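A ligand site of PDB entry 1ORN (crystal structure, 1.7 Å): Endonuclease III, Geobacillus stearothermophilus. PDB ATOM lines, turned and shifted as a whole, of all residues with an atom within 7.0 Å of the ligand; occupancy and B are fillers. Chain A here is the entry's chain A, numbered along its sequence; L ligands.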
ATOM      1  N   MET A  17      -8.315  -7.707 -27.658  1.00  0.00           N
ATOM      2  CA  MET A  17      -6.864  -7.856 -27.745  1.00  0.00           C
ATOM      3  C   MET A  17      -6.373  -7.177 -29.007  1.00  0.00           C
ATOM      4  O   MET A  17      -5.265  -6.636 -29.042  1.00  0.00           O
ATOM      5  CB  MET A  17      -6.472  -9.337 -27.779  1.00  0.00           C
ATOM      6  CG  MET A  17      -6.854 -10.125 -26.554  1.00  0.00           C
ATOM      7  SD  MET A  17      -6.285 -11.841 -26.644  1.00  0.00           S
ATOM      8  CE  MET A  17      -7.163 -12.558 -25.215  1.00  0.00           C
ATOM      9  N   VAL A 148      -2.916 -17.383 -21.435  1.00  0.00           N
ATOM     10  CA  VAL A 148      -4.017 -16.459 -21.681  1.00  0.00           C
ATOM     11  C   VAL A 148      -5.320 -17.213 -21.899  1.00  0.00           C
ATOM     12  O   VAL A 148      -6.363 -16.834 -21.356  1.00  0.00           O
ATOM     13  CB  VAL A 148      -3.726 -15.562 -22.914  1.00  0.00           C
ATOM     14  CG1 VAL A 148      -4.975 -14.799 -23.326  1.00  0.00           C
ATOM     15  CG2 VAL A 148      -2.606 -14.583 -22.571  1.00  0.00           C
ATOM     16  N   ARG A 151      -6.501 -18.686 -18.443  1.00  0.00           N
ATOM     17  CA  ARG A 151      -6.922 -17.679 -17.464  1.00  0.00           C
ATOM     18  C   ARG A 151      -8.282 -17.098 -17.831  1.00  0.00           C
ATOM     19  O   ARG A 151      -9.155 -16.944 -16.973  1.00  0.00           O
ATOM     20  CB  ARG A 151      -5.901 -16.550 -17.376  1.00  0.00           C
ATOM     21  CG  ARG A 151      -4.643 -16.912 -16.634  1.00  0.00           C
ATOM     22  CD  ARG A 151      -3.719 -15.717 -16.550  1.00  0.00           C
ATOM     23  NE  ARG A 151      -2.604 -15.946 -15.629  1.00  0.00           N
ATOM     24  CZ  ARG A 151      -1.574 -15.122 -15.475  1.00  0.00           C
ATOM     25  NH1 ARG A 151      -1.517 -14.001 -16.185  1.00  0.00           N
ATOM     26  NH2 ARG A 151      -0.623 -15.412 -14.613  1.00  0.00           N
ATOM     27  N   LEU A 152      -8.462 -16.787 -19.106  1.00  0.00           N
ATOM     28  CA  LEU A 152      -9.708 -16.202 -19.597  1.00  0.00           C
ATOM     29  C   LEU A 152     -10.872 -17.194 -19.652  1.00  0.00           C
ATOM     30  O   LEU A 152     -12.042 -16.789 -19.637  1.00  0.00           O
ATOM     31  CB  LEU A 152      -9.484 -15.610 -20.988  1.00  0.00           C
ATOM     32  CG  LEU A 152      -9.702 -14.117 -21.231  1.00  0.00           C
ATOM     33  CD1 LEU A 152      -9.756 -13.316 -19.924  1.00  0.00           C
ATOM     34  CD2 LEU A 152      -8.578 -13.615 -22.126  1.00  0.00           C
ATOM     35  N   PHE A 187      -0.645  -9.931 -25.935  1.00  0.00           N
ATOM     36  CA  PHE A 187      -1.515  -9.743 -24.773  1.00  0.00           C
ATOM     37  C   PHE A 187      -0.878 -10.404 -23.554  1.00  0.00           C
ATOM     38  O   PHE A 187      -0.810  -9.816 -22.486  1.00  0.00           O
ATOM     39  CB  PHE A 187      -2.896 -10.343 -25.051  1.00  0.00           C
ATOM     40  CG  PHE A 187      -3.898 -10.094 -23.961  1.00  0.00           C
ATOM     41  CD1 PHE A 187      -4.504  -8.842 -23.840  1.00  0.00           C
ATOM     42  CD2 PHE A 187      -4.247 -11.099 -23.071  1.00  0.00           C
ATOM     43  CE1 PHE A 187      -5.444  -8.608 -22.835  1.00  0.00           C
ATOM     44  CE2 PHE A 187      -5.186 -10.873 -22.061  1.00  0.00           C
ATOM     45  CZ  PHE A 187      -5.785  -9.623 -21.945  1.00  0.00           C
ATOM     46  N   HIS A 191       0.745  -7.725 -21.240  1.00  0.00           N
ATOM     47  CA  HIS A 191      -0.392  -7.377 -20.386  1.00  0.00           C
ATOM     48  C   HIS A 191      -0.744  -8.450 -19.366  1.00  0.00           C
ATOM     49  O   HIS A 191      -0.593  -8.258 -18.164  1.00  0.00           O
ATOM     50  CB  HIS A 191      -1.610  -7.081 -21.265  1.00  0.00           C
ATOM     51  CG  HIS A 191      -2.751  -6.467 -20.529  1.00  0.00           C
ATOM     52  ND1 HIS A 191      -2.694  -5.203 -19.969  1.00  0.00           N
ATOM     53  CD2 HIS A 191      -3.998  -6.940 -20.267  1.00  0.00           C
ATOM     54  CE1 HIS A 191      -3.858  -4.930 -19.405  1.00  0.00           C
ATOM     55  NE2 HIS A 191      -4.664  -5.961 -19.571  1.00  0.00           N
ATOM     56  N   CYS A 192      -1.212  -9.594 -19.867  1.00  0.00           N
ATOM     57  CA  CYS A 192      -1.581 -10.716 -19.002  1.00  0.00           C
ATOM     58  C   CYS A 192      -0.321 -11.518 -18.689  1.00  0.00           C
ATOM     59  O   CYS A 192      -0.249 -12.722 -18.948  1.00  0.00           O
ATOM     60  CB  CYS A 192      -2.614 -11.591 -19.709  1.00  0.00           C
ATOM     61  SG  CYS A 192      -3.407 -12.811 -18.654  1.00  0.00           S
ATOM     62  N   LYS A 193       0.669 -10.846 -18.123  1.00  0.00           N
ATOM     63  CA  LYS A 193       1.940 -11.471 -17.799  1.00  0.00           C
ATOM     64  C   LYS A 193       1.837 -12.600 -16.790  1.00  0.00           C
ATOM     65  O   LYS A 193       0.927 -12.634 -15.958  1.00  0.00           O
ATOM     66  CB  LYS A 193       2.935 -10.406 -17.307  1.00  0.00           C
ATOM     67  CG  LYS A 193       3.130  -9.273 -18.308  1.00  0.00           C
ATOM     68  CD  LYS A 193       4.146  -8.257 -17.804  1.00  0.00           C
ATOM     69  N   SER A 196       3.141 -10.703 -13.362  1.00  0.00           N
ATOM     70  CA  SER A 196       2.396  -9.491 -13.047  1.00  0.00           C
ATOM     71  C   SER A 196       1.279  -9.104 -13.991  1.00  0.00           C
ATOM     72  O   SER A 196       1.420  -8.122 -14.727  1.00  0.00           O
ATOM     73  N   PRO A 197       0.161  -9.846 -14.011  1.00  0.00           N
ATOM     74  CA  PRO A 197      -0.929  -9.475 -14.926  1.00  0.00           C
ATOM     75  C   PRO A 197      -1.525  -8.112 -14.552  1.00  0.00           C
ATOM     76  O   PRO A 197      -1.654  -7.794 -13.372  1.00  0.00           O
ATOM     77  CB  PRO A 197      -1.915 -10.630 -14.768  1.00  0.00           C
ATOM     78  CG  PRO A 197      -1.688 -11.090 -13.354  1.00  0.00           C
ATOM     79  CD  PRO A 197      -0.184 -11.050 -13.244  1.00  0.00           C
ATOM     80  N   GLN A 198      -1.877  -7.317 -15.557  1.00  0.00           N
ATOM     81  CA  GLN A 198      -2.442  -5.990 -15.344  1.00  0.00           C
ATOM     82  C   GLN A 198      -3.961  -6.013 -15.224  1.00  0.00           C
ATOM     83  O   GLN A 198      -4.658  -5.243 -15.875  1.00  0.00           O
ATOM     84  CB  GLN A 198      -2.028  -5.068 -16.493  1.00  0.00           C
ATOM     85  N   CYS A 199      -4.467  -6.889 -14.357  1.00  0.00           N
ATOM     86  CA  CYS A 199      -5.901  -7.052 -14.134  1.00  0.00           C
ATOM     87  C   CYS A 199      -6.677  -5.752 -13.861  1.00  0.00           C
ATOM     88  O   CYS A 199      -7.681  -5.460 -14.511  1.00  0.00           O
ATOM     89  CB  CYS A 199      -6.137  -8.045 -12.986  1.00  0.00           C
ATOM     90  SG  CYS A 199      -5.270  -9.641 -13.149  1.00  0.00           S
ATOM     91  N   PRO A 200      -6.210  -4.944 -12.896  1.00  0.00           N
ATOM     92  CA  PRO A 200      -6.872  -3.683 -12.549  1.00  0.00           C
ATOM     93  C   PRO A 200      -7.297  -2.816 -13.725  1.00  0.00           C
ATOM     94  O   PRO A 200      -8.356  -2.186 -13.695  1.00  0.00           O
ATOM     95  CB  PRO A 200      -5.836  -2.987 -11.664  1.00  0.00           C
ATOM     96  CG  PRO A 200      -5.224  -4.145 -10.933  1.00  0.00           C
ATOM     97  CD  PRO A 200      -5.018  -5.157 -12.048  1.00  0.00           C
ATOM     98  N   SER A 201      -6.485  -2.792 -14.772  1.00  0.00           N
ATOM     99  CA  SER A 201      -6.777  -1.979 -15.950  1.00  0.00           C
ATOM    100  C   SER A 201      -7.144  -2.829 -17.171  1.00  0.00           C
ATOM    101  O   SER A 201      -7.127  -2.334 -18.290  1.00  0.00           O
ATOM    102  CB  SER A 201      -5.577  -1.110 -16.291  1.00  0.00           C
ATOM    103  OG  SER A 201      -4.438  -1.923 -16.559  1.00  0.00           O
ATOM    104  N   CYS A 202      -7.483  -4.090 -16.946  1.00  0.00           N
ATOM    105  CA  CYS A 202      -7.811  -4.981 -18.059  1.00  0.00           C
ATOM    106  C   CYS A 202      -9.251  -4.860 -18.549  1.00  0.00           C
ATOM    107  O   CYS A 202     -10.201  -4.952 -17.776  1.00  0.00           O
ATOM    108  CB  CYS A 202      -7.525  -6.428 -17.657  1.00  0.00           C
ATOM    109  SG  CYS A 202      -7.704  -7.581 -19.043  1.00  0.00           S
ATOM    110  N   PRO A 203      -9.422  -4.659 -19.863  1.00  0.00           N
ATOM    111  CA  PRO A 203     -10.729  -4.523 -20.527  1.00  0.00           C
ATOM    112  C   PRO A 203     -11.548  -5.814 -20.494  1.00  0.00           C
ATOM    113  O   PRO A 203     -12.729  -5.809 -20.851  1.00  0.00           O
ATOM    114  CB  PRO A 203     -10.360  -4.121 -21.947  1.00  0.00           C
ATOM    115  CG  PRO A 203      -9.026  -3.458 -21.798  1.00  0.00           C
ATOM    116  CD  PRO A 203      -8.335  -4.362 -20.816  1.00  0.00           C
ATOM    117  N   LEU A 204     -10.921  -6.905 -20.073  1.00  0.00           N
ATOM    118  CA  LEU A 204     -11.596  -8.196 -20.028  1.00  0.00           C
ATOM    119  C   LEU A 204     -11.831  -8.669 -18.602  1.00  0.00           C
ATOM    120  O   LEU A 204     -12.352  -9.758 -18.378  1.00  0.00           O
ATOM    121  CB  LEU A 204     -10.766  -9.244 -20.785  1.00  0.00           C
ATOM    122  CG  LEU A 204     -10.561  -8.978 -22.274  1.00  0.00           C
ATOM    123  CD1 LEU A 204      -9.626 -10.043 -22.849  1.00  0.00           C
ATOM    124  CD2 LEU A 204     -11.909  -8.982 -23.004  1.00  0.00           C
ATOM    125  N   LEU A 205     -11.455  -7.837 -17.635  1.00  0.00           N
ATOM    126  CA  LEU A 205     -11.633  -8.167 -16.229  1.00  0.00           C
ATOM    127  C   LEU A 205     -13.092  -8.552 -15.948  1.00  0.00           C
ATOM    128  O   LEU A 205     -13.356  -9.448 -15.151  1.00  0.00           O
ATOM    129  CB  LEU A 205     -11.255  -6.952 -15.356  1.00  0.00           C
ATOM    130  CG  LEU A 205     -10.703  -7.170 -13.942  1.00  0.00           C
ATOM    131  CD1 LEU A 205     -10.964  -5.901 -13.126  1.00  0.00           C
ATOM    132  CD2 LEU A 205     -11.336  -8.363 -13.263  1.00  0.00           C
ATOM    133  N   HIS A 206     -14.030  -7.876 -16.616  1.00  0.00           N
ATOM    134  CA  HIS A 206     -15.466  -8.133 -16.419  1.00  0.00           C
ATOM    135  C   HIS A 206     -15.963  -9.538 -16.762  1.00  0.00           C
ATOM    136  O   HIS A 206     -17.114  -9.865 -16.481  1.00  0.00           O
ATOM    137  CB  HIS A 206     -16.291  -7.115 -17.219  1.00  0.00           C
ATOM    138  CG  HIS A 206     -16.281  -7.353 -18.695  1.00  0.00           C
ATOM    139  ND1 HIS A 206     -15.259  -6.935 -19.513  1.00  0.00           N
ATOM    140  CD2 HIS A 206     -17.172  -7.987 -19.494  1.00  0.00           C
ATOM    141  CE1 HIS A 206     -15.522  -7.285 -20.754  1.00  0.00           C
ATOM    142  NE2 HIS A 206     -16.671  -7.931 -20.779  1.00  0.00           N
ATOM    143  N   LEU A 207     -15.112 -10.347 -17.370  1.00  0.00           N
ATOM    144  CA  LEU A 207     -15.508 -11.713 -17.705  1.00  0.00           C
ATOM    145  C   LEU A 207     -14.419 -12.725 -17.409  1.00  0.00           C
ATOM    146  O   LEU A 207     -14.563 -13.907 -17.707  1.00  0.00           O
ATOM    147  CB  LEU A 207     -15.912 -11.810 -19.189  1.00  0.00           C
ATOM    148  CG  LEU A 207     -14.979 -11.350 -20.318  1.00  0.00           C
ATOM    149  CD1 LEU A 207     -13.636 -12.062 -20.243  1.00  0.00           C
ATOM    150  CD2 LEU A 207     -15.660 -11.640 -21.656  1.00  0.00           C
ATOM    151  N   CYS A 208     -13.325 -12.266 -16.796  1.00  0.00           N
ATOM    152  CA  CYS A 208     -12.215 -13.158 -16.492  1.00  0.00           C
ATOM    153  C   CYS A 208     -12.243 -13.797 -15.103  1.00  0.00           C
ATOM    154  O   CYS A 208     -12.215 -13.107 -14.093  1.00  0.00           O
ATOM    155  CB  CYS A 208     -10.890 -12.428 -16.691  1.00  0.00           C
ATOM    156  SG  CYS A 208      -9.460 -13.497 -16.451  1.00  0.00           S
ATOM    157  N   ARG A 209     -12.281 -15.127 -15.080  1.00  0.00           N
ATOM    158  CA  ARG A 209     -12.305 -15.872 -13.829  1.00  0.00           C
ATOM    159  C   ARG A 209     -11.028 -15.662 -13.039  1.00  0.00           C
ATOM    160  O   ARG A 209     -11.049 -15.535 -11.815  1.00  0.00           O
ATOM    161  CB  ARG A 209     -12.498 -17.358 -14.113  1.00  0.00           C
ATOM    162  N   GLU A 210      -9.902 -15.621 -13.752  1.00  0.00           N
ATOM    163  CA  GLU A 210      -8.591 -15.424 -13.125  1.00  0.00           C
ATOM    164  C   GLU A 210      -8.442 -14.006 -12.592  1.00  0.00           C
ATOM    165  O   GLU A 210      -7.961 -13.795 -11.471  1.00  0.00           O
ATOM    166  CB  GLU A 210      -7.491 -15.697 -14.152  1.00  0.00           C
ATOM    167  CG  GLU A 210      -6.073 -15.514 -13.618  1.00  0.00           C
ATOM    168  CD  GLU A 210      -5.683 -16.591 -12.641  1.00  0.00           C
ATOM    169  OE1 GLU A 210      -4.605 -16.465 -12.009  1.00  0.00           O
ATOM    170  OE2 GLU A 210      -6.445 -17.572 -12.503  1.00  0.00           O
ATOM    171  N   GLY A 211      -8.848 -13.030 -13.393  1.00  0.00           N
ATOM    172  CA  GLY A 211      -8.753 -11.638 -12.985  1.00  0.00           C
ATOM    173  C   GLY A 211      -9.573 -11.331 -11.736  1.00  0.00           C
ATOM    174  O   GLY A 211      -9.059 -10.742 -10.789  1.00  0.00           O
ATOM    175  N   LYS A 212     -10.837 -11.741 -11.741  1.00  0.00           N
ATOM    176  CA  LYS A 212     -11.699 -11.508 -10.583  1.00  0.00           C
ATOM    177  C   LYS A 212     -11.153 -12.202  -9.342  1.00  0.00           C
ATOM    178  O   LYS A 212     -11.284 -11.704  -8.228  1.00  0.00           O
ATOM    179  CB  LYS A 212     -13.125 -12.007 -10.873  1.00  0.00           C
ATOM    180  CG  LYS A 212     -13.795 -11.338 -12.071  1.00  0.00           C
ATOM    181  CD  LYS A 212     -15.214 -11.847 -12.274  1.00  0.00           C
ATOM    182  CE  LYS A 212     -15.789 -11.385 -13.606  1.00  0.00           C
ATOM    183  NZ  LYS A 212     -15.861  -9.897 -13.737  1.00  0.00           N
ATOM    184  N   ARG A 214      -7.978 -12.724  -8.702  1.00  0.00           N
ATOM    185  CA  ARG A 214      -6.800 -11.985  -8.244  1.00  0.00           C
ATOM    186  C   ARG A 214      -7.202 -10.664  -7.602  1.00  0.00           C
ATOM    187  O   ARG A 214      -6.643 -10.258  -6.579  1.00  0.00           O
ATOM    188  CB  ARG A 214      -5.848 -11.729  -9.419  1.00  0.00           C
ATOM    189  CG  ARG A 214      -5.053 -12.944  -9.859  1.00  0.00           C
ATOM    190  CD  ARG A 214      -4.304 -12.684 -11.157  1.00  0.00           C
ATOM    191  NE  ARG A 214      -3.440 -13.808 -11.524  1.00  0.00           N
ATOM    192  CZ  ARG A 214      -2.286 -14.098 -10.926  1.00  0.00           C
ATOM    193  NH1 ARG A 214      -1.850 -13.349  -9.914  1.00  0.00           N
ATOM    194  NH2 ARG A 214      -1.563 -15.137 -11.316  1.00  0.00           N
ATOM    195  N   MET A 215      -8.179  -9.980  -8.202  1.00  0.00           N
ATOM    196  CA  MET A 215      -8.647  -8.706  -7.678  1.00  0.00           C
ATOM    197  C   MET A 215      -9.205  -8.886  -6.270  1.00  0.00           C
ATOM    198  O   MET A 215      -9.010  -8.033  -5.398  1.00  0.00           O
ATOM    199  CB  MET A 215      -9.718  -8.105  -8.592  1.00  0.00           C
ATOM    200  CG  MET A 215      -9.187  -7.671  -9.964  1.00  0.00           C
ATOM    201  SD  MET A 215      -7.960  -6.358  -9.871  1.00  0.00           S
ATOM    202  CE  MET A 215      -9.017  -4.893 -10.002  1.00  0.00           C
HETATM  203 FE1  LIG L   1      -6.985  -9.448 -17.848  1.00  0.00          FE
HETATM  204 FE2  LIG L   1      -5.212 -11.562 -17.685  1.00  0.00          FE
HETATM  205 FE3  LIG L   1      -6.009 -10.235 -15.511  1.00  0.00          FE
HETATM  206 FE4  LIG L   1      -7.743 -11.807 -16.875  1.00  0.00          FE
HETATM  207  S1  LIG L   1      -5.915 -12.528 -15.688  1.00  0.00           S
HETATM  208  S2  LIG L   1      -8.143  -9.855 -15.939  1.00  0.00           S
HETATM  209  S3  LIG L   1      -6.964 -11.525 -18.941  1.00  0.00           S
HETATM  210  S4  LIG L   1      -4.776  -9.367 -17.121  1.00  0.00           S
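SG of Cys 202 lies close to NE2 of His 191 (3.5 Å). The side-chain sulfur of Cys 202 sits close to the backbone NH of Leu 204. N of Cys 192 sits at hydrogen-bond distance from O of Phe 187 (2.7 Å). The side-chain sulfur (SG) of Cys 208 sits close to the backbone NH (N) of Gly 211, at 3.2 Å. SG of Cys 208 lies close to N of Glu 210, at 3.5 Å. SG of Cys 208 lies close to O of Arg 151, at 3.5 Å. The guanidinium group (NE) of Arg 214 is in salt-bridge range of the side-chain carboxylate (OE1) of Glu 210 (2.9 Å). The backbone carbonyl oxygen (O) of Leu 205 lies within hydrogen-bond range of the side-chain amino group (NZ) of Lys 212 (2.9 Å).
Arg 151 touches the ligand. CD1 of Leu 152 touches S3 of the ligand, at 3.5 Å. CE2 of Phe 187 touches S3 of the ligand (3.6 Å). Pro 197 touches the ligand (CB to S4, 3.9 Å). N of Gln 198 touches S4 of the ligand (3.9 Å). Leu 205 touches the ligand (CA to S2, 3.9 Å). Glu 210 touches the ligand (CG to S1, 3.6 Å). Hydrophobic or aromatic side chains that line the ligand: Leu 152, Phe 187 and Pro 197. Within 4 Å of the ligand: Arg 151, Leu 152, Phe 187, Cys 192, Pro 197, Gln 198, Cys 199, Cys 202, Leu 205, Cys 208, Glu 210 and Gly 211.
The side-chain sulfur (SG) of Cys 202 is bound to an iron atom (FE1) of the ligand (2.3 Å). The side-chain sulfur of Cys 192 binds an iron atom (FE2) of the ligand. The side-chain sulfur (SG) of Cys 208 is bound to an iron atom (FE4) of the ligand (2.4 Å). N of Cys 199 sits close to S4 of the ligand, at 3.7 Å. An iron atom (FE3) of the ligand is bound by the side-chain sulfur of Cys 199, at 2.5 Å. The backbone NH (N) of Gly 211 lies close to a sulfur (S1) of the ligand, 3.8 Å away.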
